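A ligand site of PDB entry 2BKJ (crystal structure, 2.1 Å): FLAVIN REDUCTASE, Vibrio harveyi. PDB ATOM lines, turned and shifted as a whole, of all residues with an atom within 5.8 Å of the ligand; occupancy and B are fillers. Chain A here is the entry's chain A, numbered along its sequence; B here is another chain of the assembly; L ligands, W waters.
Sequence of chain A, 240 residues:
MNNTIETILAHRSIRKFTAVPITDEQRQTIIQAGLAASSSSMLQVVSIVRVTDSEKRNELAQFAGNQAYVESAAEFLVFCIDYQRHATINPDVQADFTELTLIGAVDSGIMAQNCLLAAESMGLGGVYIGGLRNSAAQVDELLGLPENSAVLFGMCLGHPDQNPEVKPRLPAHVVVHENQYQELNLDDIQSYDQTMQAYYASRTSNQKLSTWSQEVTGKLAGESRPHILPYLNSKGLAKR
Water W1 lies within hydrogen-bond range of O7 of the ligand (2.6 Å), O of His 11 (2.8 Å) and N of Lys 167 (2.9 Å). Water W3 bridges the backbone carbonyl oxygen of Glu 165 (2.9 Å) and an oxygen (O8) of the ligand (2.9 Å). Water W2 bridges NH1 of Arg 15 (3.0 Å) and O8 of the ligand (3.1 Å). Water W4 lies within hydrogen-bond range of the side-chain hydroxyl (OG) of Ser 40 of chain B and the guanidinium group (NH2) of Arg 133. Water W5 lies within hydrogen-bond range of O of Ser 13 (2.8 Å), NH1 of Arg 15 (3.3 Å) and O8 of the ligand (3.5 Å).
O8 of the ligand sits at hydrogen-bond distance from N of Ser 13 (2.7 Å). The side-chain hydroxyl (OG) of Ser 13 lies within hydrogen-bond range of an oxygen (O9) of the ligand. NE of Arg 15 sits at hydrogen-bond distance from O1 of the ligand (2.7 Å). An oxygen (O7) of the ligand lies within salt-bridge range of the guanidinium group (NH2) of Arg 169 (2.8 Å). The side-chain amide oxygen (OE1) of Gln 67 is in hydrogen-bond range of a nitrogen (N2) of the ligand, 2.8 Å away. N3 of the ligand sits at hydrogen-bond distance from N of Gly 130, at 2.9 Å. A ring nitrogen (NE2) of His 11 sits at hydrogen-bond distance from an oxygen (O9) of the ligand, 2.9 Å away. The backbone NH of Ser 39 of chain B lies within hydrogen-bond range of an oxygen (O4) of the ligand, 3.0 Å away. The backbone carbonyl oxygen of Ser 39 of chain B lies within hydrogen-bond range of an oxygen (O4) of the ligand (3.3 Å). The side-chain hydroxyl (OH) of Tyr 69 lies within hydrogen-bond range of an oxygen (O1) of the ligand (3.1 Å). An oxygen (O2) of the ligand lies within hydrogen-bond range of the backbone NH (N) of Gly 131 (3.2 Å). NZ of Lys 167 is in hydrogen-bond range of O5 of the ligand (3.3 Å).
NH1 of Arg 169 lies within hydrogen-bond range of O of Lys 167 (2.9 Å). NH2 of Arg 169 lies within hydrogen-bond range of O of Ala 37 of chain B (2.9 Å). The side-chain hydroxyl (OH) of Tyr 69 is in hydrogen-bond range of the side-chain amide oxygen (OE1) of Gln 67. NE2 of Gln 67 sits at hydrogen-bond distance from O of Ala 64 (2.8 Å). NE2 of His 11 is in hydrogen-bond range of OG of Ser 38 of chain B. The side-chain hydroxyl of Ser 40 of chain B sits at hydrogen-bond distance from the side-chain carboxylate of Asp 107 of chain B (2.8 Å).
The backbone carbonyl oxygen of Tyr 128 lies close to a nitrogen (N3) of the ligand (3.1 Å). Residues that only touch the ligand: Ser 40 of chain B (3.2 Å), Ser 38 of chain B (3.3 Å), Arg 12 (3.4 Å), Ile 129 (3.5 Å), Val 127 (3.6 Å), Met 42 of chain B (3.6 Å), Asp 107 of chain B (3.6 Å), Ile 110 of chain B (3.7 Å) and Val 106 of chain B (3.9 Å). Hydrophobic or aromatic side chains within 4 Å of the ligand: His 11, Tyr 69, Val 127, Tyr 128, Ile 129, Met 42 of chain B, Val 106 of chain B and Ile 110 of chain B. Within 4 Å of the ligand: His 11, Arg 12, Ser 13, Arg 15, Gln 67, Tyr 69, Val 127, Tyr 128, Ile 129, Gly 130, Gly 131, Lys 167, Arg 169, Ser 38 of chain B, Ser 39 of chain B, Ser 40 of chain B, Met 42 of chain B, Val 106 of chain B, Asp 107 of chain B and Ile 110 of chain B.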
ATOM      1  N   HIS A  11       9.288  17.866  -0.502  1.00  0.00           N
ATOM      2  CA  HIS A  11       9.473  19.160  -1.160  1.00  0.00           C
ATOM      3  C   HIS A  11      10.895  19.594  -1.493  1.00  0.00           C
ATOM      4  O   HIS A  11      11.846  19.346  -0.745  1.00  0.00           O
ATOM      5  CB  HIS A  11       8.800  20.284  -0.351  1.00  0.00           C
ATOM      6  CG  HIS A  11       9.202  21.661  -0.784  1.00  0.00           C
ATOM      7  ND1 HIS A  11       8.703  22.261  -1.924  1.00  0.00           N
ATOM      8  CD2 HIS A  11      10.104  22.528  -0.282  1.00  0.00           C
ATOM      9  CE1 HIS A  11       9.287  23.430  -2.106  1.00  0.00           C
ATOM     10  NE2 HIS A  11      10.137  23.621  -1.117  1.00  0.00           N
ATOM     11  N   ARG A  12      10.995  20.296  -2.619  1.00  0.00           N
ATOM     12  CA  ARG A  12      12.228  20.888  -3.138  1.00  0.00           C
ATOM     13  C   ARG A  12      11.774  21.815  -4.267  1.00  0.00           C
ATOM     14  O   ARG A  12      10.883  21.469  -5.042  1.00  0.00           O
ATOM     15  CB  ARG A  12      13.220  19.835  -3.653  1.00  0.00           C
ATOM     16  CG  ARG A  12      12.678  18.957  -4.747  1.00  0.00           C
ATOM     17  CD  ARG A  12      12.658  17.509  -4.306  1.00  0.00           C
ATOM     18  NE  ARG A  12      11.655  16.751  -5.060  1.00  0.00           N
ATOM     19  CZ  ARG A  12      11.746  16.484  -6.356  1.00  0.00           C
ATOM     20  NH1 ARG A  12      12.786  16.902  -7.066  1.00  0.00           N
ATOM     21  NH2 ARG A  12      10.767  15.827  -6.956  1.00  0.00           N
ATOM     22  N   SER A  13      12.313  23.019  -4.286  1.00  0.00           N
ATOM     23  CA  SER A  13      11.971  24.005  -5.306  1.00  0.00           C
ATOM     24  C   SER A  13      12.403  23.538  -6.690  1.00  0.00           C
ATOM     25  O   SER A  13      13.535  23.097  -6.874  1.00  0.00           O
ATOM     26  CB  SER A  13      12.628  25.355  -4.990  1.00  0.00           C
ATOM     27  OG  SER A  13      12.109  25.904  -3.787  1.00  0.00           O
ATOM     28  N   ARG A  15      13.025  24.631 -10.524  1.00  0.00           N
ATOM     29  CA  ARG A  15      13.297  25.812 -11.340  1.00  0.00           C
ATOM     30  C   ARG A  15      13.471  25.545 -12.837  1.00  0.00           C
ATOM     31  O   ARG A  15      13.972  26.399 -13.567  1.00  0.00           O
ATOM     32  CB  ARG A  15      14.514  26.558 -10.777  1.00  0.00           C
ATOM     33  CG  ARG A  15      14.303  27.057  -9.358  1.00  0.00           C
ATOM     34  CD  ARG A  15      15.541  27.719  -8.795  1.00  0.00           C
ATOM     35  NE  ARG A  15      15.328  28.225  -7.440  1.00  0.00           N
ATOM     36  CZ  ARG A  15      15.508  27.506  -6.331  1.00  0.00           C
ATOM     37  NH1 ARG A  15      15.918  26.247  -6.400  1.00  0.00           N
ATOM     38  NH2 ARG A  15      15.297  28.060  -5.152  1.00  0.00           N
ATOM     39  N   ALA A  64      11.750  40.132 -11.822  1.00  0.00           N
ATOM     40  CA  ALA A  64      12.062  39.181 -10.765  1.00  0.00           C
ATOM     41  C   ALA A  64      13.570  38.997 -10.659  1.00  0.00           C
ATOM     42  O   ALA A  64      14.062  38.289  -9.780  1.00  0.00           O
ATOM     43  CB  ALA A  64      11.386  37.846 -11.038  1.00  0.00           C
ATOM     44  N   GLN A  67      14.740  35.838 -13.813  1.00  0.00           N
ATOM     45  CA  GLN A  67      14.587  34.445 -13.424  1.00  0.00           C
ATOM     46  C   GLN A  67      13.740  33.794 -14.531  1.00  0.00           C
ATOM     47  O   GLN A  67      12.517  33.928 -14.547  1.00  0.00           O
ATOM     48  CB  GLN A  67      13.915  34.334 -12.050  1.00  0.00           C
ATOM     49  CG  GLN A  67      14.742  34.963 -10.921  1.00  0.00           C
ATOM     50  CD  GLN A  67      14.194  34.664  -9.528  1.00  0.00           C
ATOM     51  OE1 GLN A  67      14.047  33.504  -9.148  1.00  0.00           O
ATOM     52  NE2 GLN A  67      13.901  35.710  -8.775  1.00  0.00           N
ATOM     53  N   TYR A  69      12.606  30.842 -15.267  1.00  0.00           N
ATOM     54  CA  TYR A  69      11.482  29.954 -14.948  1.00  0.00           C
ATOM     55  C   TYR A  69      10.145  30.653 -14.766  1.00  0.00           C
ATOM     56  O   TYR A  69       9.096  29.998 -14.755  1.00  0.00           O
ATOM     57  CB  TYR A  69      11.818  29.061 -13.751  1.00  0.00           C
ATOM     58  CG  TYR A  69      12.781  29.671 -12.761  1.00  0.00           C
ATOM     59  CD1 TYR A  69      14.155  29.637 -13.006  1.00  0.00           C
ATOM     60  CD2 TYR A  69      12.329  30.292 -11.604  1.00  0.00           C
ATOM     61  CE1 TYR A  69      15.056  30.203 -12.112  1.00  0.00           C
ATOM     62  CE2 TYR A  69      13.220  30.864 -10.703  1.00  0.00           C
ATOM     63  CZ  TYR A  69      14.583  30.816 -10.961  1.00  0.00           C
ATOM     64  OH  TYR A  69      15.484  31.381 -10.082  1.00  0.00           O
ATOM     65  N   VAL A 127       8.022  26.873  -7.264  1.00  0.00           N
ATOM     66  CA  VAL A 127       8.954  27.686  -6.508  1.00  0.00           C
ATOM     67  C   VAL A 127       8.377  29.085  -6.264  1.00  0.00           C
ATOM     68  O   VAL A 127       7.727  29.662  -7.137  1.00  0.00           O
ATOM     69  CB  VAL A 127      10.329  27.791  -7.234  1.00  0.00           C
ATOM     70  CG1 VAL A 127      10.191  28.496  -8.571  1.00  0.00           C
ATOM     71  CG2 VAL A 127      11.356  28.507  -6.353  1.00  0.00           C
ATOM     72  N   TYR A 128       8.569  29.597  -5.049  1.00  0.00           N
ATOM     73  CA  TYR A 128       8.097  30.941  -4.695  1.00  0.00           C
ATOM     74  C   TYR A 128       9.028  31.951  -5.348  1.00  0.00           C
ATOM     75  O   TYR A 128      10.219  31.682  -5.492  1.00  0.00           O
ATOM     76  CB  TYR A 128       8.135  31.155  -3.176  1.00  0.00           C
ATOM     77  CG  TYR A 128       7.083  30.427  -2.394  1.00  0.00           C
ATOM     78  CD1 TYR A 128       7.280  29.110  -1.975  1.00  0.00           C
ATOM     79  CD2 TYR A 128       5.904  31.066  -2.025  1.00  0.00           C
ATOM     80  CE1 TYR A 128       6.327  28.447  -1.203  1.00  0.00           C
ATOM     81  CE2 TYR A 128       4.940  30.417  -1.253  1.00  0.00           C
ATOM     82  CZ  TYR A 128       5.157  29.114  -0.849  1.00  0.00           C
ATOM     83  OH  TYR A 128       4.213  28.458  -0.085  1.00  0.00           O
ATOM     84  N   ILE A 129       8.505  33.100  -5.733  1.00  0.00           N
ATOM     85  CA  ILE A 129       9.316  34.136  -6.368  1.00  0.00           C
ATOM     86  C   ILE A 129       9.179  35.446  -5.601  1.00  0.00           C
ATOM     87  O   ILE A 129       8.257  36.228  -5.836  1.00  0.00           O
ATOM     88  CB  ILE A 129       8.922  34.347  -7.856  1.00  0.00           C
ATOM     89  CG1 ILE A 129       9.019  33.029  -8.644  1.00  0.00           C
ATOM     90  CG2 ILE A 129       9.813  35.406  -8.501  1.00  0.00           C
ATOM     91  CD1 ILE A 129      10.415  32.466  -8.765  1.00  0.00           C
ATOM     92  N   GLY A 130      10.097  35.673  -4.664  1.00  0.00           N
ATOM     93  CA  GLY A 130      10.092  36.893  -3.879  1.00  0.00           C
ATOM     94  C   GLY A 130      10.861  38.021  -4.548  1.00  0.00           C
ATOM     95  O   GLY A 130      10.826  39.161  -4.094  1.00  0.00           O
ATOM     96  N   GLY A 131      11.560  37.687  -5.645  1.00  0.00           N
ATOM     97  CA  GLY A 131      12.339  38.666  -6.377  1.00  0.00           C
ATOM     98  C   GLY A 131      11.539  39.830  -6.931  1.00  0.00           C
ATOM     99  O   GLY A 131      12.092  40.899  -7.197  1.00  0.00           O
ATOM    100  N   LEU A 132      10.236  39.622  -7.098  1.00  0.00           N
ATOM    101  CA  LEU A 132       9.340  40.664  -7.612  1.00  0.00           C
ATOM    102  C   LEU A 132       9.368  41.914  -6.743  1.00  0.00           C
ATOM    103  O   LEU A 132       9.161  43.025  -7.253  1.00  0.00           O
ATOM    104  CB  LEU A 132       7.906  40.129  -7.702  1.00  0.00           C
ATOM    105  CG  LEU A 132       7.612  39.001  -8.690  1.00  0.00           C
ATOM    106  CD1 LEU A 132       6.151  38.615  -8.589  1.00  0.00           C
ATOM    107  CD2 LEU A 132       7.957  39.431 -10.112  1.00  0.00           C
ATOM    108  N   ARG A 133       9.625  41.742  -5.449  1.00  0.00           N
ATOM    109  CA  ARG A 133       9.667  42.866  -4.509  1.00  0.00           C
ATOM    110  C   ARG A 133      10.792  43.867  -4.730  1.00  0.00           C
ATOM    111  O   ARG A 133      10.718  45.007  -4.261  1.00  0.00           O
ATOM    112  CB  ARG A 133       9.684  42.365  -3.049  1.00  0.00           C
ATOM    113  CG  ARG A 133       8.380  41.722  -2.591  1.00  0.00           C
ATOM    114  CD  ARG A 133       8.272  41.672  -1.073  1.00  0.00           C
ATOM    115  NE  ARG A 133       9.416  41.017  -0.443  1.00  0.00           N
ATOM    116  CZ  ARG A 133       9.572  39.697  -0.348  1.00  0.00           C
ATOM    117  NH1 ARG A 133       8.659  38.865  -0.857  1.00  0.00           N
ATOM    118  NH2 ARG A 133      10.641  39.203   0.249  1.00  0.00           N
ATOM    119  N   PHE A 153       4.677  38.335  -3.458  1.00  0.00           N
ATOM    120  CA  PHE A 153       5.493  37.327  -4.130  1.00  0.00           C
ATOM    121  C   PHE A 153       4.729  36.586  -5.218  1.00  0.00           C
ATOM    122  O   PHE A 153       3.497  36.607  -5.247  1.00  0.00           O
ATOM    123  CB  PHE A 153       6.045  36.317  -3.116  1.00  0.00           C
ATOM    124  CG  PHE A 153       4.984  35.602  -2.319  1.00  0.00           C
ATOM    125  CD1 PHE A 153       4.367  34.457  -2.815  1.00  0.00           C
ATOM    126  CD2 PHE A 153       4.587  36.097  -1.078  1.00  0.00           C
ATOM    127  CE1 PHE A 153       3.372  33.807  -2.084  1.00  0.00           C
ATOM    128  CE2 PHE A 153       3.592  35.447  -0.333  1.00  0.00           C
ATOM    129  CZ  PHE A 153       2.985  34.302  -0.843  1.00  0.00           C
ATOM    130  N   GLU A 165      17.979  17.401  -5.050  1.00  0.00           N
ATOM    131  CA  GLU A 165      17.954  16.665  -3.792  1.00  0.00           C
ATOM    132  C   GLU A 165      17.324  17.558  -2.722  1.00  0.00           C
ATOM    133  O   GLU A 165      17.349  18.788  -2.844  1.00  0.00           O
ATOM    134  CB  GLU A 165      19.386  16.282  -3.385  1.00  0.00           C
ATOM    135  N   LYS A 167      16.960  19.732   0.361  1.00  0.00           N
ATOM    136  CA  LYS A 167      17.861  20.594   1.125  1.00  0.00           C
ATOM    137  C   LYS A 167      17.634  20.457   2.634  1.00  0.00           C
ATOM    138  O   LYS A 167      16.507  20.609   3.109  1.00  0.00           O
ATOM    139  CB  LYS A 167      17.633  22.059   0.756  1.00  0.00           C
ATOM    140  CG  LYS A 167      18.715  22.703  -0.070  1.00  0.00           C
ATOM    141  CD  LYS A 167      18.508  24.213  -0.058  1.00  0.00           C
ATOM    142  CE  LYS A 167      19.188  24.897  -1.231  1.00  0.00           C
ATOM    143  NZ  LYS A 167      19.004  26.380  -1.163  1.00  0.00           N
ATOM    144  N   ARG A 169      17.542  21.397   6.621  1.00  0.00           N
ATOM    145  CA  ARG A 169      17.226  22.605   7.382  1.00  0.00           C
ATOM    146  C   ARG A 169      17.933  22.554   8.731  1.00  0.00           C
ATOM    147  O   ARG A 169      18.513  21.527   9.093  1.00  0.00           O
ATOM    148  CB  ARG A 169      15.712  22.693   7.644  1.00  0.00           C
ATOM    149  CG  ARG A 169      14.924  23.522   6.647  1.00  0.00           C
ATOM    150  CD  ARG A 169      14.869  22.884   5.287  1.00  0.00           C
ATOM    151  NE  ARG A 169      13.869  23.512   4.440  1.00  0.00           N
ATOM    152  CZ  ARG A 169      13.904  23.534   3.108  1.00  0.00           C
ATOM    153  NH1 ARG A 169      14.903  22.961   2.462  1.00  0.00           N
ATOM    154  NH2 ARG A 169      12.930  24.128   2.437  1.00  0.00           N
ATOM    155  N   ALA B  36      10.196  21.493   6.641  1.00  0.00           N
ATOM    156  CA  ALA B  36      10.283  21.169   5.218  1.00  0.00           C
ATOM    157  C   ALA B  36       9.713  22.257   4.311  1.00  0.00           C
ATOM    158  O   ALA B  36       9.744  22.131   3.087  1.00  0.00           O
ATOM    159  CB  ALA B  36       9.597  19.840   4.938  1.00  0.00           C
ATOM    160  N   ALA B  37       9.204  23.333   4.909  1.00  0.00           N
ATOM    161  CA  ALA B  37       8.629  24.444   4.164  1.00  0.00           C
ATOM    162  C   ALA B  37       9.703  25.300   3.493  1.00  0.00           C
ATOM    163  O   ALA B  37      10.838  25.366   3.964  1.00  0.00           O
ATOM    164  CB  ALA B  37       7.785  25.311   5.093  1.00  0.00           C
ATOM    165  N   SER B  38       9.334  25.960   2.391  1.00  0.00           N
ATOM    166  CA  SER B  38      10.255  26.835   1.661  1.00  0.00           C
ATOM    167  C   SER B  38      10.705  27.979   2.559  1.00  0.00           C
ATOM    168  O   SER B  38       9.956  28.423   3.430  1.00  0.00           O
ATOM    169  CB  SER B  38       9.582  27.403   0.414  1.00  0.00           C
ATOM    170  OG  SER B  38       9.307  26.403  -0.547  1.00  0.00           O
ATOM    171  N   SER B  39      11.920  28.459   2.338  1.00  0.00           N
ATOM    172  CA  SER B  39      12.478  29.548   3.133  1.00  0.00           C
ATOM    173  C   SER B  39      13.059  30.622   2.223  1.00  0.00           C
ATOM    174  O   SER B  39      13.825  30.312   1.315  1.00  0.00           O
ATOM    175  CB  SER B  39      13.551  29.014   4.084  1.00  0.00           C
ATOM    176  OG  SER B  39      14.128  30.054   4.844  1.00  0.00           O
ATOM    177  N   SER B  40      12.696  31.875   2.468  1.00  0.00           N
ATOM    178  CA  SER B  40      13.179  33.004   1.673  1.00  0.00           C
ATOM    179  C   SER B  40      14.692  33.130   1.778  1.00  0.00           C
ATOM    180  O   SER B  40      15.234  33.386   2.847  1.00  0.00           O
ATOM    181  CB  SER B  40      12.532  34.303   2.133  1.00  0.00           C
ATOM    182  OG  SER B  40      11.134  34.292   1.925  1.00  0.00           O
ATOM    183  N   SER B  41      15.377  32.945   0.645  1.00  0.00           N
ATOM    184  CA  SER B  41      16.834  33.027   0.553  1.00  0.00           C
ATOM    185  C   SER B  41      17.514  32.083   1.541  1.00  0.00           C
ATOM    186  O   SER B  41      18.683  32.261   1.882  1.00  0.00           O
ATOM    187  CB  SER B  41      17.308  34.458   0.804  1.00  0.00           C
ATOM    188  OG  SER B  41      16.701  35.362  -0.101  1.00  0.00           O
ATOM    189  N   MET B  42      16.776  31.061   1.975  1.00  0.00           N
ATOM    190  CA  MET B  42      17.266  30.063   2.920  1.00  0.00           C
ATOM    191  C   MET B  42      17.728  30.736   4.223  1.00  0.00           C
ATOM    192  O   MET B  42      18.620  30.254   4.911  1.00  0.00           O
ATOM    193  CB  MET B  42      18.390  29.245   2.293  1.00  0.00           C
ATOM    194  CG  MET B  42      18.677  27.924   2.999  1.00  0.00           C
ATOM    195  SD  MET B  42      17.188  26.916   3.147  1.00  0.00           S
ATOM    196  CE  MET B  42      17.902  25.354   3.635  1.00  0.00           C
ATOM    197  N   VAL B 106       5.627  36.219   6.096  1.00  0.00           N
ATOM    198  CA  VAL B 106       5.306  35.295   5.016  1.00  0.00           C
ATOM    199  C   VAL B 106       5.821  33.891   5.304  1.00  0.00           C
ATOM    200  O   VAL B 106       5.065  32.930   5.251  1.00  0.00           O
ATOM    201  CB  VAL B 106       5.883  35.786   3.670  1.00  0.00           C
ATOM    202  CG1 VAL B 106       5.705  34.716   2.593  1.00  0.00           C
ATOM    203  CG2 VAL B 106       5.195  37.073   3.233  1.00  0.00           C
ATOM    204  N   ASP B 107       7.115  33.789   5.629  1.00  0.00           N
ATOM    205  CA  ASP B 107       7.727  32.493   5.921  1.00  0.00           C
ATOM    206  C   ASP B 107       7.090  31.781   7.121  1.00  0.00           C
ATOM    207  O   ASP B 107       7.022  30.563   7.145  1.00  0.00           O
ATOM    208  CB  ASP B 107       9.243  32.641   6.117  1.00  0.00           C
ATOM    209  CG  ASP B 107       9.985  32.894   4.810  1.00  0.00           C
ATOM    210  OD1 ASP B 107       9.343  33.316   3.810  1.00  0.00           O
ATOM    211  OD2 ASP B 107      11.208  32.668   4.763  1.00  0.00           O
ATOM    212  N   ILE B 110       3.827  30.154   5.960  1.00  0.00           N
ATOM    213  CA  ILE B 110       4.130  28.981   5.151  1.00  0.00           C
ATOM    214  C   ILE B 110       4.472  27.782   6.045  1.00  0.00           C
ATOM    215  O   ILE B 110       3.934  26.683   5.857  1.00  0.00           O
ATOM    216  CB  ILE B 110       5.335  29.237   4.217  1.00  0.00           C
ATOM    217  CG1 ILE B 110       5.013  30.386   3.259  1.00  0.00           C
ATOM    218  CG2 ILE B 110       5.691  27.973   3.442  1.00  0.00           C
ATOM    219  CD1 ILE B 110       6.156  30.755   2.341  1.00  0.00           C
HETATM  220  N1  LIG L   1      13.669  30.924  -5.066  1.00  0.00           N
HETATM  221  C1  LIG L   1      14.039  31.433  -6.298  1.00  0.00           C
HETATM  222  O1  LIG L   1      14.694  30.790  -7.109  1.00  0.00           O
HETATM  223  N2  LIG L   1      13.639  32.740  -6.519  1.00  0.00           N
HETATM  224  C2  LIG L   1      12.974  33.554  -5.610  1.00  0.00           C
HETATM  225  O2  LIG L   1      12.733  34.715  -5.942  1.00  0.00           O
HETATM  226  C3  LIG L   1      12.638  32.890  -4.364  1.00  0.00           C
HETATM  227  N3  LIG L   1      11.761  33.608  -3.568  1.00  0.00           N
HETATM  228  C4  LIG L   1      11.259  32.983  -2.457  1.00  0.00           C
HETATM  229  C5  LIG L   1      10.291  33.648  -1.750  1.00  0.00           C
HETATM  230  C6  LIG L   1       9.688  33.028  -0.672  1.00  0.00           C
HETATM  231  C7  LIG L   1       8.458  33.682  -0.005  1.00  0.00           C
HETATM  232  C8  LIG L   1      10.124  31.765  -0.268  1.00  0.00           C
HETATM  233  C9  LIG L   1       9.516  31.075   0.938  1.00  0.00           C
HETATM  234  C10 LIG L   1      11.112  31.128  -0.948  1.00  0.00           C
HETATM  235  C11 LIG L   1      11.665  31.705  -2.081  1.00  0.00           C
HETATM  236  N4  LIG L   1      12.582  31.009  -2.844  1.00  0.00           N
HETATM  237  C12 LIG L   1      12.992  31.576  -4.035  1.00  0.00           C
HETATM  238  C13 LIG L   1      12.640  29.667  -2.710  1.00  0.00           C
HETATM  239  C14 LIG L   1      13.994  29.043  -2.341  1.00  0.00           C
HETATM  240  O3  LIG L   1      15.095  29.940  -2.171  1.00  0.00           O
HETATM  241  C15 LIG L   1      13.897  27.865  -1.376  1.00  0.00           C
HETATM  242  O4  LIG L   1      12.745  27.836  -0.530  1.00  0.00           O
HETATM  243  C16 LIG L   1      15.188  27.276  -0.786  1.00  0.00           C
HETATM  244  O5  LIG L   1      16.267  28.096  -0.410  1.00  0.00           O
HETATM  245  C17 LIG L   1      14.999  26.111   0.112  1.00  0.00           C
HETATM  246  O6  LIG L   1      15.016  25.031  -0.816  1.00  0.00           O
HETATM  247  P1  LIG L   1      13.777  24.137  -1.228  1.00  0.00           P
HETATM  248  O7  LIG L   1      13.682  23.229  -0.066  1.00  0.00           O
HETATM  249  O8  LIG L   1      14.255  23.523  -2.493  1.00  0.00           O
HETATM  250  O9  LIG L   1      12.625  25.049  -1.379  1.00  0.00           O
HETATM  251  O   HOH W   1      14.273  20.665  -0.184  1.00  0.00           O
HETATM  252  O   HOH W   2      16.316  25.541  -3.558  1.00  0.00           O
HETATM  253  O   HOH W   3      16.245  21.469  -3.021  1.00  0.00           O
HETATM  254  O   HOH W   4      10.665  36.360   0.068  1.00  0.00           O
HETATM  255  O   HOH W   5      15.973  23.070  -5.505  1.00  0.00           O
